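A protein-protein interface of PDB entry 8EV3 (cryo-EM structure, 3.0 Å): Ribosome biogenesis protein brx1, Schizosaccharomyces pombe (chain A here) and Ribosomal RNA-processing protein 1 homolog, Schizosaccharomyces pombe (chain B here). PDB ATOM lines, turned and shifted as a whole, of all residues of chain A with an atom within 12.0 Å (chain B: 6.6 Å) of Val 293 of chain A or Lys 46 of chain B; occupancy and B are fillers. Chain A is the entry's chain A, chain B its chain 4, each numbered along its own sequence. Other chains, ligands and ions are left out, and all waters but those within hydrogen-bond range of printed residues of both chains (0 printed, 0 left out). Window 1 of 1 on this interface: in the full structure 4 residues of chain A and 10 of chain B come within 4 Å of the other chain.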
ATOM      1  N   GLU A 287      19.003  -5.626 -39.253  1.00  0.00           N
ATOM      2  CA  GLU A 287      17.823  -5.132 -38.554  1.00  0.00           C
ATOM      3  C   GLU A 287      18.155  -4.203 -37.387  1.00  0.00           C
ATOM      4  O   GLU A 287      17.363  -3.302 -37.088  1.00  0.00           O
ATOM      5  CB  GLU A 287      16.983  -6.313 -38.060  1.00  0.00           C
ATOM      6  CG  GLU A 287      15.768  -5.926 -37.228  1.00  0.00           C
ATOM      7  CD  GLU A 287      14.908  -4.870 -37.899  1.00  0.00           C
ATOM      8  OE1 GLU A 287      14.726  -4.938 -39.134  1.00  0.00           O
ATOM      9  OE2 GLU A 287      14.422  -3.963 -37.191  1.00  0.00           O
ATOM     10  N   ASP A 288      19.309  -4.390 -36.729  1.00  0.00           N
ATOM     11  CA  ASP A 288      19.648  -3.638 -35.520  1.00  0.00           C
ATOM     12  C   ASP A 288      18.595  -3.882 -34.446  1.00  0.00           C
ATOM     13  O   ASP A 288      17.745  -3.016 -34.200  1.00  0.00           O
ATOM     14  CB  ASP A 288      19.785  -2.140 -35.807  1.00  0.00           C
ATOM     15  CG  ASP A 288      20.466  -1.388 -34.677  1.00  0.00           C
ATOM     16  OD1 ASP A 288      20.686  -1.983 -33.603  1.00  0.00           O
ATOM     17  OD2 ASP A 288      20.776  -0.192 -34.861  1.00  0.00           O
ATOM     18  N   PRO A 289      18.612  -5.051 -33.796  1.00  0.00           N
ATOM     19  CA  PRO A 289      17.502  -5.432 -32.903  1.00  0.00           C
ATOM     20  C   PRO A 289      17.224  -4.456 -31.768  1.00  0.00           C
ATOM     21  O   PRO A 289      16.219  -4.631 -31.068  1.00  0.00           O
ATOM     22  CB  PRO A 289      17.950  -6.792 -32.356  1.00  0.00           C
ATOM     23  CG  PRO A 289      19.435  -6.750 -32.440  1.00  0.00           C
ATOM     24  CD  PRO A 289      19.747  -5.980 -33.689  1.00  0.00           C
ATOM     25  N   LEU A 290      18.068  -3.451 -31.551  1.00  0.00           N
ATOM     26  CA  LEU A 290      17.781  -2.414 -30.570  1.00  0.00           C
ATOM     27  C   LEU A 290      16.847  -1.339 -31.110  1.00  0.00           C
ATOM     28  O   LEU A 290      16.770  -0.250 -30.530  1.00  0.00           O
ATOM     29  CB  LEU A 290      19.083  -1.779 -30.076  1.00  0.00           C
ATOM     30  CG  LEU A 290      20.040  -2.710 -29.333  1.00  0.00           C
ATOM     31  CD1 LEU A 290      21.327  -1.993 -28.996  1.00  0.00           C
ATOM     32  CD2 LEU A 290      19.385  -3.232 -28.074  1.00  0.00           C
ATOM     33  N   ASP A 291      16.142  -1.615 -32.207  1.00  0.00           N
ATOM     34  CA  ASP A 291      15.235  -0.650 -32.813  1.00  0.00           C
ATOM     35  C   ASP A 291      13.770  -0.928 -32.507  1.00  0.00           C
ATOM     36  O   ASP A 291      12.944  -0.021 -32.646  1.00  0.00           O
ATOM     37  CB  ASP A 291      15.435  -0.623 -34.332  1.00  0.00           C
ATOM     38  CG  ASP A 291      16.210   0.595 -34.796  1.00  0.00           C
ATOM     39  OD1 ASP A 291      16.729   1.338 -33.937  1.00  0.00           O
ATOM     40  OD2 ASP A 291      16.307   0.803 -36.026  1.00  0.00           O
ATOM     41  N   ASN A 292      13.432  -2.150 -32.101  1.00  0.00           N
ATOM     42  CA  ASN A 292      12.078  -2.513 -31.714  1.00  0.00           C
ATOM     43  C   ASN A 292      11.943  -2.540 -30.191  1.00  0.00           C
ATOM     44  O   ASN A 292      10.961  -3.059 -29.662  1.00  0.00           O
ATOM     45  CB  ASN A 292      11.721  -3.867 -32.354  1.00  0.00           C
ATOM     46  CG  ASN A 292      10.221  -4.199 -32.325  1.00  0.00           C
ATOM     47  OD1 ASN A 292       9.582  -4.446 -33.343  1.00  0.00           O
ATOM     48  ND2 ASN A 292       9.661  -4.200 -31.121  1.00  0.00           N
ATOM     49  N   VAL A 293      12.917  -1.974 -29.477  1.00  0.00           N
ATOM     50  CA  VAL A 293      12.899  -2.024 -28.018  1.00  0.00           C
ATOM     51  C   VAL A 293      11.692  -1.272 -27.466  1.00  0.00           C
ATOM     52  O   VAL A 293      11.002  -1.757 -26.561  1.00  0.00           O
ATOM     53  CB  VAL A 293      14.229  -1.487 -27.457  1.00  0.00           C
ATOM     54  CG1 VAL A 293      14.595  -0.166 -28.107  1.00  0.00           C
ATOM     55  CG2 VAL A 293      14.159  -1.343 -25.960  1.00  0.00           C
ATOM     56  N   PHE A 294      11.403  -0.086 -28.008  1.00  0.00           N
ATOM     57  CA  PHE A 294      10.222   0.668 -27.609  1.00  0.00           C
ATOM     58  C   PHE A 294       9.050   0.496 -28.563  1.00  0.00           C
ATOM     59  O   PHE A 294       7.917   0.814 -28.188  1.00  0.00           O
ATOM     60  CB  PHE A 294      10.544   2.162 -27.497  1.00  0.00           C
ATOM     61  CG  PHE A 294      11.652   2.476 -26.538  1.00  0.00           C
ATOM     62  CD1 PHE A 294      11.523   2.194 -25.193  1.00  0.00           C
ATOM     63  CD2 PHE A 294      12.819   3.066 -26.983  1.00  0.00           C
ATOM     64  CE1 PHE A 294      12.542   2.486 -24.315  1.00  0.00           C
ATOM     65  CE2 PHE A 294      13.837   3.359 -26.109  1.00  0.00           C
ATOM     66  CZ  PHE A 294      13.698   3.070 -24.774  1.00  0.00           C
ATOM     67  N   ALA A 295       9.291   0.009 -29.774  1.00  0.00           N
ATOM     68  CA  ALA A 295       8.238  -0.132 -30.770  1.00  0.00           C
ATOM     69  C   ALA A 295       7.302  -1.287 -30.443  1.00  0.00           C
ATOM     70  O   ALA A 295       6.562  -1.756 -31.304  1.00  0.00           O
ATOM     71  CB  ALA A 295       8.845  -0.320 -32.149  1.00  0.00           C
ATOM     72  OXT ALA A 295       7.264  -1.789 -29.321  1.00  0.00           O
ATOM     73  N   ILE B   8      10.718  -2.336 -20.403  1.00  0.00           N
ATOM     74  CA  ILE B   8      11.591  -1.282 -20.902  1.00  0.00           C
ATOM     75  C   ILE B   8      10.764  -0.100 -21.388  1.00  0.00           C
ATOM     76  O   ILE B   8      11.136   1.061 -21.189  1.00  0.00           O
ATOM     77  CB  ILE B   8      12.523  -1.816 -22.010  1.00  0.00           C
ATOM     78  CG1 ILE B   8      13.596  -2.794 -21.489  1.00  0.00           C
ATOM     79  CG2 ILE B   8      13.207  -0.670 -22.710  1.00  0.00           C
ATOM     80  CD1 ILE B   8      13.131  -4.002 -20.699  1.00  0.00           C
ATOM     81  N   LYS B   9       9.625  -0.378 -22.026  1.00  0.00           N
ATOM     82  CA  LYS B   9       8.755   0.695 -22.498  1.00  0.00           C
ATOM     83  C   LYS B   9       8.277   1.575 -21.351  1.00  0.00           C
ATOM     84  O   LYS B   9       8.084   2.782 -21.534  1.00  0.00           O
ATOM     85  CB  LYS B   9       7.564   0.101 -23.251  1.00  0.00           C
ATOM     86  CG  LYS B   9       7.068   0.944 -24.411  1.00  0.00           C
ATOM     87  CD  LYS B   9       6.119   0.151 -25.287  1.00  0.00           C
ATOM     88  CE  LYS B   9       5.302   1.062 -26.185  1.00  0.00           C
ATOM     89  NZ  LYS B   9       6.167   1.893 -27.058  1.00  0.00           N
ATOM     90  N   ALA B  12      10.940   4.297 -20.067  1.00  0.00           N
ATOM     91  CA  ALA B  12      11.089   5.505 -20.867  1.00  0.00           C
ATOM     92  C   ALA B  12       9.745   6.190 -21.091  1.00  0.00           C
ATOM     93  O   ALA B  12       9.497   6.776 -22.144  1.00  0.00           O
ATOM     94  CB  ALA B  12      11.754   5.188 -22.203  1.00  0.00           C
ATOM     95  N   PHE B  41      20.410  -7.578 -21.763  1.00  0.00           N
ATOM     96  CA  PHE B  41      20.863  -6.430 -20.988  1.00  0.00           C
ATOM     97  C   PHE B  41      21.023  -5.192 -21.858  1.00  0.00           C
ATOM     98  O   PHE B  41      20.821  -4.071 -21.380  1.00  0.00           O
ATOM     99  CB  PHE B  41      22.178  -6.758 -20.289  1.00  0.00           C
ATOM    100  CG  PHE B  41      22.006  -7.443 -18.969  1.00  0.00           C
ATOM    101  CD1 PHE B  41      20.775  -7.482 -18.349  1.00  0.00           C
ATOM    102  CD2 PHE B  41      23.079  -8.049 -18.347  1.00  0.00           C
ATOM    103  CE1 PHE B  41      20.619  -8.112 -17.135  1.00  0.00           C
ATOM    104  CE2 PHE B  41      22.925  -8.678 -17.134  1.00  0.00           C
ATOM    105  CZ  PHE B  41      21.695  -8.710 -16.528  1.00  0.00           C
ATOM    106  N   LEU B  42      21.398  -5.370 -23.125  1.00  0.00           N
ATOM    107  CA  LEU B  42      21.518  -4.230 -24.027  1.00  0.00           C
ATOM    108  C   LEU B  42      20.171  -3.557 -24.245  1.00  0.00           C
ATOM    109  O   LEU B  42      20.085  -2.326 -24.292  1.00  0.00           O
ATOM    110  CB  LEU B  42      22.114  -4.676 -25.360  1.00  0.00           C
ATOM    111  CG  LEU B  42      23.634  -4.792 -25.424  1.00  0.00           C
ATOM    112  CD1 LEU B  42      24.068  -5.228 -26.808  1.00  0.00           C
ATOM    113  CD2 LEU B  42      24.280  -3.478 -25.050  1.00  0.00           C
ATOM    114  N   LYS B  43      19.108  -4.350 -24.401  1.00  0.00           N
ATOM    115  CA  LYS B  43      17.772  -3.777 -24.508  1.00  0.00           C
ATOM    116  C   LYS B  43      17.327  -3.173 -23.184  1.00  0.00           C
ATOM    117  O   LYS B  43      16.662  -2.133 -23.162  1.00  0.00           O
ATOM    118  CB  LYS B  43      16.777  -4.837 -24.972  1.00  0.00           C
ATOM    119  CG  LYS B  43      17.143  -5.496 -26.282  1.00  0.00           C
ATOM    120  CD  LYS B  43      16.358  -6.773 -26.486  1.00  0.00           C
ATOM    121  CE  LYS B  43      15.235  -6.562 -27.476  1.00  0.00           C
ATOM    122  NZ  LYS B  43      15.747  -6.051 -28.773  1.00  0.00           N
ATOM    123  N   LEU B  44      17.676  -3.819 -22.071  1.00  0.00           N
ATOM    124  CA  LEU B  44      17.343  -3.275 -20.761  1.00  0.00           C
ATOM    125  C   LEU B  44      18.036  -1.940 -20.528  1.00  0.00           C
ATOM    126  O   LEU B  44      17.455  -1.025 -19.935  1.00  0.00           O
ATOM    127  CB  LEU B  44      17.718  -4.277 -19.671  1.00  0.00           C
ATOM    128  CG  LEU B  44      17.555  -3.837 -18.218  1.00  0.00           C
ATOM    129  CD1 LEU B  44      16.740  -4.859 -17.454  1.00  0.00           C
ATOM    130  CD2 LEU B  44      18.910  -3.647 -17.564  1.00  0.00           C
ATOM    131  N   TRP B  45      19.277  -1.809 -20.991  1.00  0.00           N
ATOM    132  CA  TRP B  45      20.015  -0.565 -20.835  1.00  0.00           C
ATOM    133  C   TRP B  45      19.613   0.497 -21.846  1.00  0.00           C
ATOM    134  O   TRP B  45      20.063   1.639 -21.727  1.00  0.00           O
ATOM    135  CB  TRP B  45      21.517  -0.829 -20.927  1.00  0.00           C
ATOM    136  CG  TRP B  45      22.138  -1.037 -19.592  1.00  0.00           C
ATOM    137  CD1 TRP B  45      22.710  -2.178 -19.126  1.00  0.00           C
ATOM    138  CD2 TRP B  45      22.240  -0.076 -18.537  1.00  0.00           C
ATOM    139  NE1 TRP B  45      23.168  -1.990 -17.848  1.00  0.00           N
ATOM    140  CE2 TRP B  45      22.890  -0.705 -17.462  1.00  0.00           C
ATOM    141  CE3 TRP B  45      21.846   1.257 -18.400  1.00  0.00           C
ATOM    142  CZ2 TRP B  45      23.155  -0.051 -16.268  1.00  0.00           C
ATOM    143  CZ3 TRP B  45      22.107   1.904 -17.213  1.00  0.00           C
ATOM    144  CH2 TRP B  45      22.754   1.251 -16.162  1.00  0.00           C
ATOM    145  N   LYS B  46      18.794   0.154 -22.838  1.00  0.00           N
ATOM    146  CA  LYS B  46      18.218   1.182 -23.696  1.00  0.00           C
ATOM    147  C   LYS B  46      17.113   1.938 -22.968  1.00  0.00           C
ATOM    148  O   LYS B  46      17.004   3.161 -23.095  1.00  0.00           O
ATOM    149  CB  LYS B  46      17.690   0.554 -24.984  1.00  0.00           C
ATOM    150  CG  LYS B  46      17.272   1.555 -26.036  1.00  0.00           C
ATOM    151  CD  LYS B  46      18.447   1.988 -26.884  1.00  0.00           C
ATOM    152  CE  LYS B  46      17.982   2.768 -28.099  1.00  0.00           C
ATOM    153  NZ  LYS B  46      19.091   3.526 -28.738  1.00  0.00           N
ATOM    154  N   GLY B  47      16.279   1.225 -22.211  1.00  0.00           N
ATOM    155  CA  GLY B  47      15.293   1.895 -21.380  1.00  0.00           C
ATOM    156  C   GLY B  47      15.914   2.638 -20.214  1.00  0.00           C
ATOM    157  O   GLY B  47      15.509   3.757 -19.893  1.00  0.00           O
ATOM    158  N   LEU B  48      16.908   2.027 -19.564  1.00  0.00           N
ATOM    159  CA  LEU B  48      17.552   2.661 -18.418  1.00  0.00           C
ATOM    160  C   LEU B  48      18.326   3.906 -18.823  1.00  0.00           C
ATOM    161  O   LEU B  48      18.408   4.862 -18.045  1.00  0.00           O
ATOM    162  CB  LEU B  48      18.479   1.672 -17.721  1.00  0.00           C
ATOM    163  CG  LEU B  48      17.822   0.660 -16.791  1.00  0.00           C
ATOM    164  CD1 LEU B  48      18.872  -0.207 -16.136  1.00  0.00           C
ATOM    165  CD2 LEU B  48      17.007   1.385 -15.753  1.00  0.00           C
ATOM    166  N   PHE B  49      18.921   3.906 -20.015  1.00  0.00           N
ATOM    167  CA  PHE B  49      19.567   5.115 -20.510  1.00  0.00           C
ATOM    168  C   PHE B  49      18.552   6.229 -20.702  1.00  0.00           C
ATOM    169  O   PHE B  49      18.833   7.393 -20.400  1.00  0.00           O
ATOM    170  CB  PHE B  49      20.297   4.821 -21.821  1.00  0.00           C
ATOM    171  CG  PHE B  49      20.597   6.044 -22.641  1.00  0.00           C
ATOM    172  CD1 PHE B  49      21.743   6.780 -22.412  1.00  0.00           C
ATOM    173  CD2 PHE B  49      19.742   6.449 -23.650  1.00  0.00           C
ATOM    174  CE1 PHE B  49      22.019   7.897 -23.166  1.00  0.00           C
ATOM    175  CE2 PHE B  49      20.015   7.569 -24.397  1.00  0.00           C
ATOM    176  CZ  PHE B  49      21.152   8.290 -24.156  1.00  0.00           C
ATOM    177  N   TYR B  50      17.369   5.895 -21.214  1.00  0.00           N
ATOM    178  CA  TYR B  50      16.337   6.897 -21.437  1.00  0.00           C
ATOM    179  C   TYR B  50      15.571   7.243 -20.171  1.00  0.00           C
ATOM    180  O   TYR B  50      14.965   8.316 -20.107  1.00  0.00           O
ATOM    181  CB  TYR B  50      15.377   6.422 -22.524  1.00  0.00           C
ATOM    182  CG  TYR B  50      15.828   6.824 -23.903  1.00  0.00           C
ATOM    183  CD1 TYR B  50      15.991   8.158 -24.234  1.00  0.00           C
ATOM    184  CD2 TYR B  50      16.112   5.872 -24.867  1.00  0.00           C
ATOM    185  CE1 TYR B  50      16.410   8.534 -25.482  1.00  0.00           C
ATOM    186  CE2 TYR B  50      16.532   6.239 -26.122  1.00  0.00           C
ATOM    187  CZ  TYR B  50      16.678   7.574 -26.423  1.00  0.00           C
ATOM    188  OH  TYR B  50      17.097   7.953 -27.676  1.00  0.00           O
ATOM    189  N   CYS B  51      15.576   6.367 -19.169  1.00  0.00           N
ATOM    190  CA  CYS B  51      15.083   6.765 -17.856  1.00  0.00           C
ATOM    191  C   CYS B  51      15.964   7.857 -17.266  1.00  0.00           C
ATOM    192  O   CYS B  51      15.468   8.792 -16.630  1.00  0.00           O
ATOM    193  CB  CYS B  51      15.025   5.550 -16.932  1.00  0.00           C
ATOM    194  SG  CYS B  51      14.535   5.896 -15.231  1.00  0.00           S
ATOM    195  N   THR B  90      26.410   0.862 -24.031  1.00  0.00           N
ATOM    196  CA  THR B  90      25.366   1.818 -24.373  1.00  0.00           C
ATOM    197  C   THR B  90      25.752   3.251 -24.050  1.00  0.00           C
ATOM    198  O   THR B  90      25.138   4.177 -24.584  1.00  0.00           O
ATOM    199  CB  THR B  90      24.063   1.479 -23.650  1.00  0.00           C
ATOM    200  OG1 THR B  90      24.174   1.843 -22.271  1.00  0.00           O
ATOM    201  CG2 THR B  90      23.757   0.002 -23.762  1.00  0.00           C
ATOM    202  N   ARG B  93      27.987   4.185 -27.441  1.00  0.00           N
ATOM    203  CA  ARG B  93      27.262   4.368 -28.688  1.00  0.00           C
ATOM    204  C   ARG B  93      26.251   5.501 -28.631  1.00  0.00           C
ATOM    205  O   ARG B  93      25.779   5.938 -29.684  1.00  0.00           O
ATOM    206  CB  ARG B  93      26.554   3.073 -29.080  1.00  0.00           C
ATOM    207  CG  ARG B  93      25.339   2.766 -28.247  1.00  0.00           C
ATOM    208  CD  ARG B  93      24.248   2.113 -29.069  1.00  0.00           C
ATOM    209  NE  ARG B  93      23.046   1.903 -28.272  1.00  0.00           N
ATOM    210  CZ  ARG B  93      22.863   0.871 -27.462  1.00  0.00           C
ATOM    211  NH1 ARG B  93      23.771  -0.080 -27.339  1.00  0.00           N
ATOM    212  NH2 ARG B  93      21.739   0.793 -26.757  1.00  0.00           N
ATOM    213  N   GLU B  94      25.911   5.991 -27.443  1.00  0.00           N
ATOM    214  CA  GLU B  94      24.980   7.098 -27.309  1.00  0.00           C
ATOM    215  C   GLU B  94      25.627   8.359 -26.765  1.00  0.00           C
ATOM    216  O   GLU B  94      24.949   9.387 -26.674  1.00  0.00           O
ATOM    217  CB  GLU B  94      23.801   6.698 -26.414  1.00  0.00           C
ATOM    218  CG  GLU B  94      23.239   5.329 -26.723  1.00  0.00           C
ATOM    219  CD  GLU B  94      21.760   5.356 -27.034  1.00  0.00           C
ATOM    220  OE1 GLU B  94      21.311   6.304 -27.709  1.00  0.00           O
ATOM    221  OE2 GLU B  94      21.049   4.422 -26.609  1.00  0.00           O
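Among the printed residues, merely in contact across the chains: Val 293 of chain A with Ile 8 of chain B, Leu 290 of chain A with Arg 93 of chain B, Phe 294 of chain A with Ala 12 of chain B, Phe 294 of chain A with Ile 8 of chain B, Phe 294 of chain A with Tyr 50 of chain B, Leu 290 of chain A with Lys 43 of chain B, Phe 294 of chain A with Lys 46 of chain B, Val 293 of chain A with Lys 46 of chain B, Val 293 of chain A with Lys 43 of chain B, Leu 290 of chain A with Leu 42 of chain B and Phe 294 of chain A with Gly 47 of chain B.
The backbone carbonyl oxygen of Pro 289 of chain A lies within hydrogen-bond range of the side-chain amino group of Lys 43 of chain B (2.7 Å). The side-chain amino group (NZ) of Lys 9 of chain B sits close to the backbone carbonyl oxygen (O) of Phe 294 of chain A (2.3 Å).
Of the printed residues of chain B, Leu 290 of chain A touches Leu 42, Lys 43 and Arg 93. Asp 291 of chain A touches none of the printed residues of chain B. Of chain B, only Ile 8 (3.5 Å), Lys 43 (3.8 Å) and Lys 46 (3.8 Å) come within 4 Å of Val 293 of chain A. Printed residues of chain B within 4 Å of Phe 294 of chain A: Ile 8 (3.6 Å), Lys 9 (2.3 Å), Ala 12 (3.5 Å), Lys 46 (3.7 Å), Gly 47 (3.9 Å) and Tyr 50 (3.6 Å). Lys 9 of chain B touches just one residue of chain A: Phe 294. Of the printed residues of chain A, Leu 42 of chain B touches Leu 290. Of chain A, only Pro 289 (2.7 Å), Leu 290 (3.7 Å) and Val 293 (3.8 Å) come within 4 Å of Lys 43 of chain B. No residue of chain A comes within 4 Å of Leu 44 of chain B. No residue of chain A comes within 4 Å of Trp 45 of chain B. Of the printed residues of chain A, Lys 46 of chain B touches Val 293 and Phe 294. Of chain A, only Phe 294 (3.9 Å) comes within 4 Å of Gly 47 of chain B. No residue of chain A comes within 4 Å of Leu 48 of chain B. No residue of chain A comes within 4 Å of Phe 49 of chain B. Printed residues of chain A within 4 Å of Arg 93 of chain B: Leu 290 (3.5 Å). The nearest residue of chain B that does not touch Val 293 of chain A is Lys 9 of chain B (4.9 Å). The nearest residue of chain A that does not touch Lys 46 of chain B is Leu 290 of chain A (4.1 Å).
Printed residues of chain B that touch a printed residue of chain A: Ile 8, Lys 9, Ala 12, Leu 42, Lys 43, Lys 46, Gly 47, Tyr 50 and Arg 93. Of the 9 printed residues of chain A, 4 touch a printed residue of chain B. Printed residues of chain A that touch a printed residue of chain B: Pro 289, Leu 290, Val 293 and Phe 294. Along chain A the printed residues that touch a printed residue of chain B span positions 289 to 294.
OE2 of Glu 94 of chain B is in salt-bridge range of NE of Arg 93 of chain B. NZ of Lys 46 of chain B lies within salt-bridge range of OE2 of Glu 94 of chain B (3.0 Å).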
